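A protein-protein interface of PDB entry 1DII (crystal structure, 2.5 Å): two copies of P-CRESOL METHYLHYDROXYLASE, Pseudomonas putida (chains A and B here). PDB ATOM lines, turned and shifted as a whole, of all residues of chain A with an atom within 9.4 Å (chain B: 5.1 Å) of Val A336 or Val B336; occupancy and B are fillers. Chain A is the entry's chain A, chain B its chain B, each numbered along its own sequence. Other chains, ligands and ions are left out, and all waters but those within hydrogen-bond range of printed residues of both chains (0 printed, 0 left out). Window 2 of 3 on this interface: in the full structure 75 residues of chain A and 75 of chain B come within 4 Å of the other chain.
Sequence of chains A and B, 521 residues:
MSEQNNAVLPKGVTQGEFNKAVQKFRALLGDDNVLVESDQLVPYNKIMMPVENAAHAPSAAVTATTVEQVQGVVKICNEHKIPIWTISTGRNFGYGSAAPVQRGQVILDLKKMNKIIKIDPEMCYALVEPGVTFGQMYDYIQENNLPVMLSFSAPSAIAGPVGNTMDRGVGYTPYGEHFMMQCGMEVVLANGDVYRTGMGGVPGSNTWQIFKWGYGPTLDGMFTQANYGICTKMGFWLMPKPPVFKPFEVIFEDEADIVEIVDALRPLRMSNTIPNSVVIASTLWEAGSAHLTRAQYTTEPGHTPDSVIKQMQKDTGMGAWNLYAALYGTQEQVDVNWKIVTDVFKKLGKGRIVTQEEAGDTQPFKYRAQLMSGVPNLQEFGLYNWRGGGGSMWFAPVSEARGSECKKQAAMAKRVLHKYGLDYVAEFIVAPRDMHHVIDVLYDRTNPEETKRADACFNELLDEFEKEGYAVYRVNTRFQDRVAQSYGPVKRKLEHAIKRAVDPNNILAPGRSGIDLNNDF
OD1 of Asn B337 lies within hydrogen-bond range of NE2 of Gln A333 (2.9 Å). The side-chain amide nitrogen of Gln B333 sits at hydrogen-bond distance from the side-chain amide oxygen of Asn A337 (2.9 Å).
Glu A332 touches Val B336, and with the chains exchanged Val A336 touches Glu B332. Gln A333 touches Asn B337, and with the chains exchanged Asn A337 touches Gln B333. Gln A333 touches Ile B340, and with the chains exchanged Ile A340 touches Gln B333. Val B336 touches its own counterpart, Val A336. Positions printed for both chains: 331, 332, 333, 334, 335, 336, 337, 338, 339 and 340. Of the 10 pairs that touch across the chains among the printed residues, 9 have their exchanged pair printed and touching as well.
The side-chain amide oxygen (OE1) of Gln A333 is in hydrogen-bond range of the backbone NH (N) of Thr A330 (2.9 Å). O of Gln A333 is in hydrogen-bond range of ND2 of Asn A337 (3.2 Å). The backbone carbonyl oxygen (O) of Gln B333 lies within hydrogen-bond range of the side-chain amide nitrogen (ND2) of Asn B337, at 3.2 Å.
Of chain B, only Glu B332, Gln B333 and Val B336 come within 4 Å of Val A336. Of chain A, only Glu A332 (3.8 Å), Gln A333 (3.8 Å) and Val A336 (3.4 Å) come within 4 Å of Val B336. Of the printed residues of chain A, Asn B337 touches Gln A333 (2.9 Å). Printed residues of chain B within 4 Å of Gln A333: Val B336 (3.8 Å), Asn B337 (2.9 Å) and Ile B340 (3.6 Å). Of the printed residues of chain A, Ile B340 touches Thr A330 and Gln A333. Printed residues of chain A within 4 Å of Gln B333: Val A336, Asn A337 and Ile A340. Printed residues of chain B within 4 Å of Thr A330: Ile B340 (3.7 Å). Printed residues of chain B within 4 Å of Ile A340: Gln B333. The nearest printed residue of chain B that does not touch Val A336 is Val B334 (6.3 Å). The nearest printed residue of chain A that does not touch Glu B332 is Ile A340 (5.9 Å).
Of the 20 printed residues of chain A, 6 touch a printed residue of chain B. Hydrophobic or aromatic side chains of chain B within 4 Å of the printed part of chain A: Val B336 and Ile B340.
Among the printed residues, pairs that only touch across the chains: Val A336 with Val B336 (3.4 Å), Gln A333 with Ile B340 (3.6 Å), Ile A340 with Gln B333 (3.7 Å), Thr A330 with Ile B340 (3.7 Å), Val A336 with Glu B332 (3.8 Å), Glu A332 with Val B336 (3.8 Å), Gln A333 with Val B336 (3.8 Å) and Val A336 with Gln B333 (3.8 Å).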
ATOM      1  N   LYS A 246      12.799  22.260  18.728  1.00  0.00           N
ATOM      2  CA  LYS A 246      13.797  22.959  17.937  1.00  0.00           C
ATOM      3  C   LYS A 246      14.245  22.195  16.688  1.00  0.00           C
ATOM      4  O   LYS A 246      15.157  21.349  16.750  1.00  0.00           O
ATOM      5  CB  LYS A 246      15.016  23.333  18.799  1.00  0.00           C
ATOM      6  CG  LYS A 246      16.064  24.199  18.085  1.00  0.00           C
ATOM      7  CD  LYS A 246      16.814  25.096  19.061  1.00  0.00           C
ATOM      8  CE  LYS A 246      17.565  26.220  18.358  1.00  0.00           C
ATOM      9  NZ  LYS A 246      18.570  25.681  17.411  1.00  0.00           N
ATOM     10  N   LEU A 268      25.780  10.748  18.350  1.00  0.00           N
ATOM     11  CA  LEU A 268      24.795  11.715  18.852  1.00  0.00           C
ATOM     12  C   LEU A 268      23.400  11.097  18.836  1.00  0.00           C
ATOM     13  O   LEU A 268      22.546  11.436  19.649  1.00  0.00           O
ATOM     14  CB  LEU A 268      24.770  12.985  17.994  1.00  0.00           C
ATOM     15  CG  LEU A 268      25.969  13.930  17.911  1.00  0.00           C
ATOM     16  CD1 LEU A 268      25.570  15.144  17.080  1.00  0.00           C
ATOM     17  CD2 LEU A 268      26.425  14.381  19.296  1.00  0.00           C
ATOM     18  N   THR A 273      21.104  12.311  22.056  1.00  0.00           N
ATOM     19  CA  THR A 273      21.302  13.776  22.042  1.00  0.00           C
ATOM     20  C   THR A 273      20.381  14.319  20.933  1.00  0.00           C
ATOM     21  O   THR A 273      19.796  15.393  21.069  1.00  0.00           O
ATOM     22  CB  THR A 273      22.785  14.140  21.782  1.00  0.00           C
ATOM     23  OG1 THR A 273      23.597  13.451  22.737  1.00  0.00           O
ATOM     24  CG2 THR A 273      23.034  15.650  21.920  1.00  0.00           C
ATOM     25  N   LEU A 327      15.203  18.767  18.073  1.00  0.00           N
ATOM     26  CA  LEU A 327      15.585  18.745  19.484  1.00  0.00           C
ATOM     27  C   LEU A 327      14.332  18.994  20.323  1.00  0.00           C
ATOM     28  O   LEU A 327      13.504  19.816  19.960  1.00  0.00           O
ATOM     29  CB  LEU A 327      16.662  19.801  19.748  1.00  0.00           C
ATOM     30  CG  LEU A 327      18.131  19.390  19.933  1.00  0.00           C
ATOM     31  CD1 LEU A 327      18.653  18.406  18.908  1.00  0.00           C
ATOM     32  CD2 LEU A 327      18.964  20.641  19.906  1.00  0.00           C
ATOM     33  N   TYR A 328      14.141  18.187  21.375  1.00  0.00           N
ATOM     34  CA  TYR A 328      12.952  18.277  22.246  1.00  0.00           C
ATOM     35  C   TYR A 328      13.355  18.295  23.716  1.00  0.00           C
ATOM     36  O   TYR A 328      14.373  17.715  24.092  1.00  0.00           O
ATOM     37  CB  TYR A 328      11.993  17.070  22.035  1.00  0.00           C
ATOM     38  CG  TYR A 328      11.696  16.665  20.592  1.00  0.00           C
ATOM     39  CD1 TYR A 328      10.423  16.860  20.025  1.00  0.00           C
ATOM     40  CD2 TYR A 328      12.691  16.081  19.791  1.00  0.00           C
ATOM     41  CE1 TYR A 328      10.159  16.474  18.689  1.00  0.00           C
ATOM     42  CE2 TYR A 328      12.450  15.707  18.465  1.00  0.00           C
ATOM     43  CZ  TYR A 328      11.186  15.904  17.918  1.00  0.00           C
ATOM     44  OH  TYR A 328      10.989  15.557  16.606  1.00  0.00           O
ATOM     45  N   GLY A 329      12.512  18.919  24.536  1.00  0.00           N
ATOM     46  CA  GLY A 329      12.740  19.005  25.964  1.00  0.00           C
ATOM     47  C   GLY A 329      12.453  20.398  26.490  1.00  0.00           C
ATOM     48  O   GLY A 329      11.639  21.125  25.923  1.00  0.00           O
ATOM     49  N   THR A 330      13.076  20.737  27.620  1.00  0.00           N
ATOM     50  CA  THR A 330      12.941  22.054  28.236  1.00  0.00           C
ATOM     51  C   THR A 330      13.981  22.927  27.553  1.00  0.00           C
ATOM     52  O   THR A 330      14.958  22.402  27.002  1.00  0.00           O
ATOM     53  CB  THR A 330      13.214  22.030  29.770  1.00  0.00           C
ATOM     54  OG1 THR A 330      14.586  21.692  30.025  1.00  0.00           O
ATOM     55  CG2 THR A 330      12.296  21.036  30.478  1.00  0.00           C
ATOM     56  N   GLN A 331      13.795  24.247  27.627  1.00  0.00           N
ATOM     57  CA  GLN A 331      14.705  25.211  27.003  1.00  0.00           C
ATOM     58  C   GLN A 331      16.163  24.973  27.388  1.00  0.00           C
ATOM     59  O   GLN A 331      17.049  24.923  26.527  1.00  0.00           O
ATOM     60  CB  GLN A 331      14.275  26.654  27.350  1.00  0.00           C
ATOM     61  CG  GLN A 331      14.945  27.755  26.507  1.00  0.00           C
ATOM     62  CD  GLN A 331      14.726  27.571  25.010  1.00  0.00           C
ATOM     63  OE1 GLN A 331      13.626  27.803  24.500  1.00  0.00           O
ATOM     64  NE2 GLN A 331      15.769  27.131  24.305  1.00  0.00           N
ATOM     65  N   GLU A 332      16.365  24.661  28.666  1.00  0.00           N
ATOM     66  CA  GLU A 332      17.692  24.418  29.191  1.00  0.00           C
ATOM     67  C   GLU A 332      18.353  23.179  28.623  1.00  0.00           C
ATOM     68  O   GLU A 332      19.528  23.243  28.254  1.00  0.00           O
ATOM     69  CB  GLU A 332      17.686  24.407  30.721  1.00  0.00           C
ATOM     70  CG  GLU A 332      17.439  25.786  31.362  1.00  0.00           C
ATOM     71  CD  GLU A 332      15.961  26.126  31.587  1.00  0.00           C
ATOM     72  OE1 GLU A 332      15.702  27.181  32.200  1.00  0.00           O
ATOM     73  OE2 GLU A 332      15.062  25.348  31.183  1.00  0.00           O
ATOM     74  N   GLN A 333      17.594  22.085  28.457  1.00  0.00           N
ATOM     75  CA  GLN A 333      18.193  20.866  27.902  1.00  0.00           C
ATOM     76  C   GLN A 333      18.367  20.926  26.386  1.00  0.00           C
ATOM     77  O   GLN A 333      19.327  20.352  25.840  1.00  0.00           O
ATOM     78  CB  GLN A 333      17.529  19.576  28.421  1.00  0.00           C
ATOM     79  CG  GLN A 333      16.063  19.372  28.103  1.00  0.00           C
ATOM     80  CD  GLN A 333      15.344  18.487  29.119  1.00  0.00           C
ATOM     81  OE1 GLN A 333      14.118  18.454  29.161  1.00  0.00           O
ATOM     82  NE2 GLN A 333      16.102  17.779  29.947  1.00  0.00           N
ATOM     83  N   VAL A 334      17.537  21.767  25.754  1.00  0.00           N
ATOM     84  CA  VAL A 334      17.584  22.001  24.310  1.00  0.00           C
ATOM     85  C   VAL A 334      18.825  22.836  24.003  1.00  0.00           C
ATOM     86  O   VAL A 334      19.594  22.462  23.109  1.00  0.00           O
ATOM     87  CB  VAL A 334      16.298  22.710  23.793  1.00  0.00           C
ATOM     88  CG1 VAL A 334      16.461  23.173  22.336  1.00  0.00           C
ATOM     89  CG2 VAL A 334      15.109  21.748  23.880  1.00  0.00           C
ATOM     90  N   ASP A 335      19.055  23.898  24.799  1.00  0.00           N
ATOM     91  CA  ASP A 335      20.218  24.795  24.629  1.00  0.00           C
ATOM     92  C   ASP A 335      21.538  24.058  24.793  1.00  0.00           C
ATOM     93  O   ASP A 335      22.499  24.316  24.063  1.00  0.00           O
ATOM     94  CB  ASP A 335      20.171  25.981  25.600  1.00  0.00           C
ATOM     95  CG  ASP A 335      19.043  26.972  25.292  1.00  0.00           C
ATOM     96  OD1 ASP A 335      18.515  27.587  26.249  1.00  0.00           O
ATOM     97  OD2 ASP A 335      18.677  27.145  24.106  1.00  0.00           O
ATOM     98  N   VAL A 336      21.544  23.084  25.699  1.00  0.00           N
ATOM     99  CA  VAL A 336      22.722  22.263  25.967  1.00  0.00           C
ATOM    100  C   VAL A 336      22.966  21.278  24.825  1.00  0.00           C
ATOM    101  O   VAL A 336      24.106  21.144  24.362  1.00  0.00           O
ATOM    102  CB  VAL A 336      22.604  21.523  27.338  1.00  0.00           C
ATOM    103  CG1 VAL A 336      23.794  20.598  27.575  1.00  0.00           C
ATOM    104  CG2 VAL A 336      22.570  22.536  28.440  1.00  0.00           C
ATOM    105  N   ASN A 337      21.897  20.623  24.356  1.00  0.00           N
ATOM    106  CA  ASN A 337      22.015  19.674  23.246  1.00  0.00           C
ATOM    107  C   ASN A 337      22.330  20.405  21.948  1.00  0.00           C
ATOM    108  O   ASN A 337      23.025  19.856  21.077  1.00  0.00           O
ATOM    109  CB  ASN A 337      20.755  18.817  23.099  1.00  0.00           C
ATOM    110  CG  ASN A 337      20.646  17.737  24.166  1.00  0.00           C
ATOM    111  OD1 ASN A 337      21.645  17.160  24.591  1.00  0.00           O
ATOM    112  ND2 ASN A 337      19.425  17.457  24.596  1.00  0.00           N
ATOM    113  N   TRP A 338      21.892  21.671  21.868  1.00  0.00           N
ATOM    114  CA  TRP A 338      22.169  22.510  20.705  1.00  0.00           C
ATOM    115  C   TRP A 338      23.660  22.791  20.595  1.00  0.00           C
ATOM    116  O   TRP A 338      24.224  22.635  19.514  1.00  0.00           O
ATOM    117  CB  TRP A 338      21.342  23.807  20.695  1.00  0.00           C
ATOM    118  CG  TRP A 338      21.526  24.630  19.431  1.00  0.00           C
ATOM    119  CD1 TRP A 338      22.071  25.881  19.352  1.00  0.00           C
ATOM    120  CD2 TRP A 338      21.289  24.211  18.074  1.00  0.00           C
ATOM    121  NE1 TRP A 338      22.212  26.260  18.040  1.00  0.00           N
ATOM    122  CE2 TRP A 338      21.741  25.260  17.231  1.00  0.00           C
ATOM    123  CE3 TRP A 338      20.748  23.044  17.481  1.00  0.00           C
ATOM    124  CZ2 TRP A 338      21.673  25.183  15.823  1.00  0.00           C
ATOM    125  CZ3 TRP A 338      20.683  22.964  16.084  1.00  0.00           C
ATOM    126  CH2 TRP A 338      21.145  24.032  15.269  1.00  0.00           C
ATOM    127  N   LYS A 339      24.299  23.083  21.732  1.00  0.00           N
ATOM    128  CA  LYS A 339      25.743  23.337  21.793  1.00  0.00           C
ATOM    129  C   LYS A 339      26.538  22.084  21.342  1.00  0.00           C
ATOM    130  O   LYS A 339      27.481  22.197  20.552  1.00  0.00           O
ATOM    131  CB  LYS A 339      26.142  23.740  23.217  1.00  0.00           C
ATOM    132  CG  LYS A 339      27.435  24.535  23.334  1.00  0.00           C
ATOM    133  CD  LYS A 339      27.155  26.039  23.283  1.00  0.00           C
ATOM    134  CE  LYS A 339      28.405  26.864  23.598  1.00  0.00           C
ATOM    135  NZ  LYS A 339      28.137  28.337  23.608  1.00  0.00           N
ATOM    136  N   ILE A 340      26.095  20.896  21.772  1.00  0.00           N
ATOM    137  CA  ILE A 340      26.751  19.623  21.414  1.00  0.00           C
ATOM    138  C   ILE A 340      26.624  19.324  19.914  1.00  0.00           C
ATOM    139  O   ILE A 340      27.602  18.932  19.275  1.00  0.00           O
ATOM    140  CB  ILE A 340      26.195  18.409  22.248  1.00  0.00           C
ATOM    141  CG1 ILE A 340      26.313  18.702  23.749  1.00  0.00           C
ATOM    142  CG2 ILE A 340      26.979  17.105  21.925  1.00  0.00           C
ATOM    143  CD1 ILE A 340      25.789  17.603  24.659  1.00  0.00           C
ATOM    144  N   VAL A 341      25.435  19.563  19.357  1.00  0.00           N
ATOM    145  CA  VAL A 341      25.177  19.332  17.927  1.00  0.00           C
ATOM    146  C   VAL A 341      25.967  20.329  17.047  1.00  0.00           C
ATOM    147  O   VAL A 341      26.622  19.922  16.078  1.00  0.00           O
ATOM    148  CB  VAL A 341      23.635  19.342  17.629  1.00  0.00           C
ATOM    149  CG1 VAL A 341      23.344  19.246  16.138  1.00  0.00           C
ATOM    150  CG2 VAL A 341      22.980  18.161  18.318  1.00  0.00           C
ATOM    151  N   THR A 342      25.973  21.602  17.467  1.00  0.00           N
ATOM    152  CA  THR A 342      26.678  22.705  16.796  1.00  0.00           C
ATOM    153  C   THR A 342      28.191  22.453  16.708  1.00  0.00           C
ATOM    154  O   THR A 342      28.765  22.532  15.622  1.00  0.00           O
ATOM    155  CB  THR A 342      26.374  24.056  17.524  1.00  0.00           C
ATOM    156  OG1 THR A 342      25.051  24.480  17.182  1.00  0.00           O
ATOM    157  CG2 THR A 342      27.371  25.164  17.184  1.00  0.00           C
ATOM    158  N   ASP A 343      28.806  22.090  17.837  1.00  0.00           N
ATOM    159  CA  ASP A 343      30.244  21.824  17.901  1.00  0.00           C
ATOM    160  C   ASP A 343      30.715  20.646  17.047  1.00  0.00           C
ATOM    161  O   ASP A 343      31.854  20.645  16.584  1.00  0.00           O
ATOM    162  CB  ASP A 343      30.713  21.661  19.357  1.00  0.00           C
ATOM    163  CG  ASP A 343      30.613  22.967  20.173  1.00  0.00           C
ATOM    164  OD1 ASP A 343      30.835  22.919  21.404  1.00  0.00           O
ATOM    165  OD2 ASP A 343      30.306  24.041  19.601  1.00  0.00           O
ATOM    166  N   GLN B 331      28.728  16.151  31.223  1.00  0.00           N
ATOM    167  CA  GLN B 331      28.626  16.952  32.444  1.00  0.00           C
ATOM    168  C   GLN B 331      27.560  18.034  32.354  1.00  0.00           C
ATOM    169  O   GLN B 331      26.731  18.181  33.267  1.00  0.00           O
ATOM    170  CB  GLN B 331      29.987  17.562  32.806  1.00  0.00           C
ATOM    171  CG  GLN B 331      30.078  18.146  34.227  1.00  0.00           C
ATOM    172  CD  GLN B 331      29.724  17.127  35.311  1.00  0.00           C
ATOM    173  OE1 GLN B 331      30.490  16.197  35.577  1.00  0.00           O
ATOM    174  NE2 GLN B 331      28.547  17.285  35.920  1.00  0.00           N
ATOM    175  N   GLU B 332      27.499  18.662  31.182  1.00  0.00           N
ATOM    176  CA  GLU B 332      26.546  19.730  30.933  1.00  0.00           C
ATOM    177  C   GLU B 332      25.092  19.263  30.914  1.00  0.00           C
ATOM    178  O   GLU B 332      24.236  19.925  31.529  1.00  0.00           O
ATOM    179  CB  GLU B 332      26.917  20.504  29.660  1.00  0.00           C
ATOM    180  CG  GLU B 332      28.185  21.369  29.788  1.00  0.00           C
ATOM    181  CD  GLU B 332      29.488  20.635  29.445  1.00  0.00           C
ATOM    182  OE1 GLU B 332      30.550  21.304  29.444  1.00  0.00           O
ATOM    183  OE2 GLU B 332      29.468  19.410  29.165  1.00  0.00           O
ATOM    184  N   GLN B 333      24.821  18.094  30.309  1.00  0.00           N
ATOM    185  CA  GLN B 333      23.438  17.604  30.273  1.00  0.00           C
ATOM    186  C   GLN B 333      23.012  16.976  31.588  1.00  0.00           C
ATOM    187  O   GLN B 333      21.843  17.066  31.971  1.00  0.00           O
ATOM    188  CB  GLN B 333      23.120  16.755  29.026  1.00  0.00           C
ATOM    189  CG  GLN B 333      23.925  15.493  28.837  1.00  0.00           C
ATOM    190  CD  GLN B 333      24.065  15.073  27.383  1.00  0.00           C
ATOM    191  OE1 GLN B 333      24.912  14.241  27.052  1.00  0.00           O
ATOM    192  NE2 GLN B 333      23.248  15.647  26.507  1.00  0.00           N
ATOM    193  N   VAL B 334      24.001  16.497  32.346  1.00  0.00           N
ATOM    194  CA  VAL B 334      23.776  15.917  33.672  1.00  0.00           C
ATOM    195  C   VAL B 334      23.429  17.047  34.646  1.00  0.00           C
ATOM    196  O   VAL B 334      22.442  16.934  35.370  1.00  0.00           O
ATOM    197  CB  VAL B 334      25.015  15.109  34.177  1.00  0.00           C
ATOM    198  CG1 VAL B 334      24.854  14.697  35.640  1.00  0.00           C
ATOM    199  CG2 VAL B 334      25.199  13.846  33.333  1.00  0.00           C
ATOM    200  N   ASP B 335      24.186  18.153  34.588  1.00  0.00           N
ATOM    201  CA  ASP B 335      23.967  19.320  35.458  1.00  0.00           C
ATOM    202  C   ASP B 335      22.598  19.937  35.245  1.00  0.00           C
ATOM    203  O   ASP B 335      21.940  20.366  36.207  1.00  0.00           O
ATOM    204  CB  ASP B 335      25.051  20.393  35.257  1.00  0.00           C
ATOM    205  CG  ASP B 335      26.423  19.967  35.773  1.00  0.00           C
ATOM    206  OD1 ASP B 335      27.427  20.405  35.169  1.00  0.00           O
ATOM    207  OD2 ASP B 335      26.512  19.203  36.764  1.00  0.00           O
ATOM    208  N   VAL B 336      22.145  19.911  33.990  1.00  0.00           N
ATOM    209  CA  VAL B 336      20.834  20.456  33.618  1.00  0.00           C
ATOM    210  C   VAL B 336      19.705  19.548  34.118  1.00  0.00           C
ATOM    211  O   VAL B 336      18.738  20.041  34.723  1.00  0.00           O
ATOM    212  CB  VAL B 336      20.735  20.709  32.083  1.00  0.00           C
ATOM    213  CG1 VAL B 336      19.358  21.181  31.692  1.00  0.00           C
ATOM    214  CG2 VAL B 336      21.720  21.761  31.692  1.00  0.00           C
ATOM    215  N   ASN B 337      19.858  18.235  33.905  1.00  0.00           N
ATOM    216  CA  ASN B 337      18.867  17.259  34.359  1.00  0.00           C
ATOM    217  C   ASN B 337      18.859  17.189  35.876  1.00  0.00           C
ATOM    218  O   ASN B 337      17.800  16.963  36.477  1.00  0.00           O
ATOM    219  CB  ASN B 337      19.110  15.880  33.751  1.00  0.00           C
ATOM    220  CG  ASN B 337      18.720  15.816  32.293  1.00  0.00           C
ATOM    221  OD1 ASN B 337      17.774  16.468  31.859  1.00  0.00           O
ATOM    222  ND2 ASN B 337      19.451  15.024  31.526  1.00  0.00           N
ATOM    223  N   TRP B 338      20.015  17.484  36.492  1.00  0.00           N
ATOM    224  CA  TRP B 338      20.120  17.509  37.950  1.00  0.00           C
ATOM    225  C   TRP B 338      19.263  18.620  38.536  1.00  0.00           C
ATOM    226  O   TRP B 338      18.520  18.364  39.478  1.00  0.00           O
ATOM    227  CB  TRP B 338      21.574  17.592  38.445  1.00  0.00           C
ATOM    228  CG  TRP B 338      21.704  17.490  39.959  1.00  0.00           C
ATOM    229  CD1 TRP B 338      22.165  18.461  40.797  1.00  0.00           C
ATOM    230  CD2 TRP B 338      21.257  16.413  40.807  1.00  0.00           C
ATOM    231  NE1 TRP B 338      22.016  18.077  42.107  1.00  0.00           N
ATOM    232  CE2 TRP B 338      21.464  16.828  42.148  1.00  0.00           C
ATOM    233  CE3 TRP B 338      20.692  15.137  40.567  1.00  0.00           C
ATOM    234  CZ2 TRP B 338      21.125  16.018  43.253  1.00  0.00           C
ATOM    235  CZ3 TRP B 338      20.353  14.330  41.660  1.00  0.00           C
ATOM    236  CH2 TRP B 338      20.572  14.777  42.989  1.00  0.00           C
ATOM    237  N   LYS B 339      19.296  19.799  37.904  1.00  0.00           N
ATOM    238  CA  LYS B 339      18.499  20.962  38.312  1.00  0.00           C
ATOM    239  C   LYS B 339      16.986  20.656  38.209  1.00  0.00           C
ATOM    240  O   LYS B 339      16.227  20.985  39.122  1.00  0.00           O
ATOM    241  CB  LYS B 339      18.855  22.170  37.438  1.00  0.00           C
ATOM    242  CG  LYS B 339      18.547  23.542  38.038  1.00  0.00           C
ATOM    243  CD  LYS B 339      19.755  24.084  38.792  1.00  0.00           C
ATOM    244  CE  LYS B 339      19.544  25.531  39.244  1.00  0.00           C
ATOM    245  NZ  LYS B 339      20.745  26.106  39.934  1.00  0.00           N
ATOM    246  N   ILE B 340      16.578  19.954  37.141  1.00  0.00           N
ATOM    247  CA  ILE B 340      15.167  19.580  36.923  1.00  0.00           C
ATOM    248  C   ILE B 340      14.681  18.576  37.979  1.00  0.00           C
ATOM    249  O   ILE B 340      13.591  18.746  38.531  1.00  0.00           O
ATOM    250  CB  ILE B 340      14.915  19.006  35.493  1.00  0.00           C
ATOM    251  CG1 ILE B 340      15.390  20.002  34.433  1.00  0.00           C
ATOM    252  CG2 ILE B 340      13.411  18.722  35.276  1.00  0.00           C
ATOM    253  CD1 ILE B 340      15.216  19.550  32.998  1.00  0.00           C
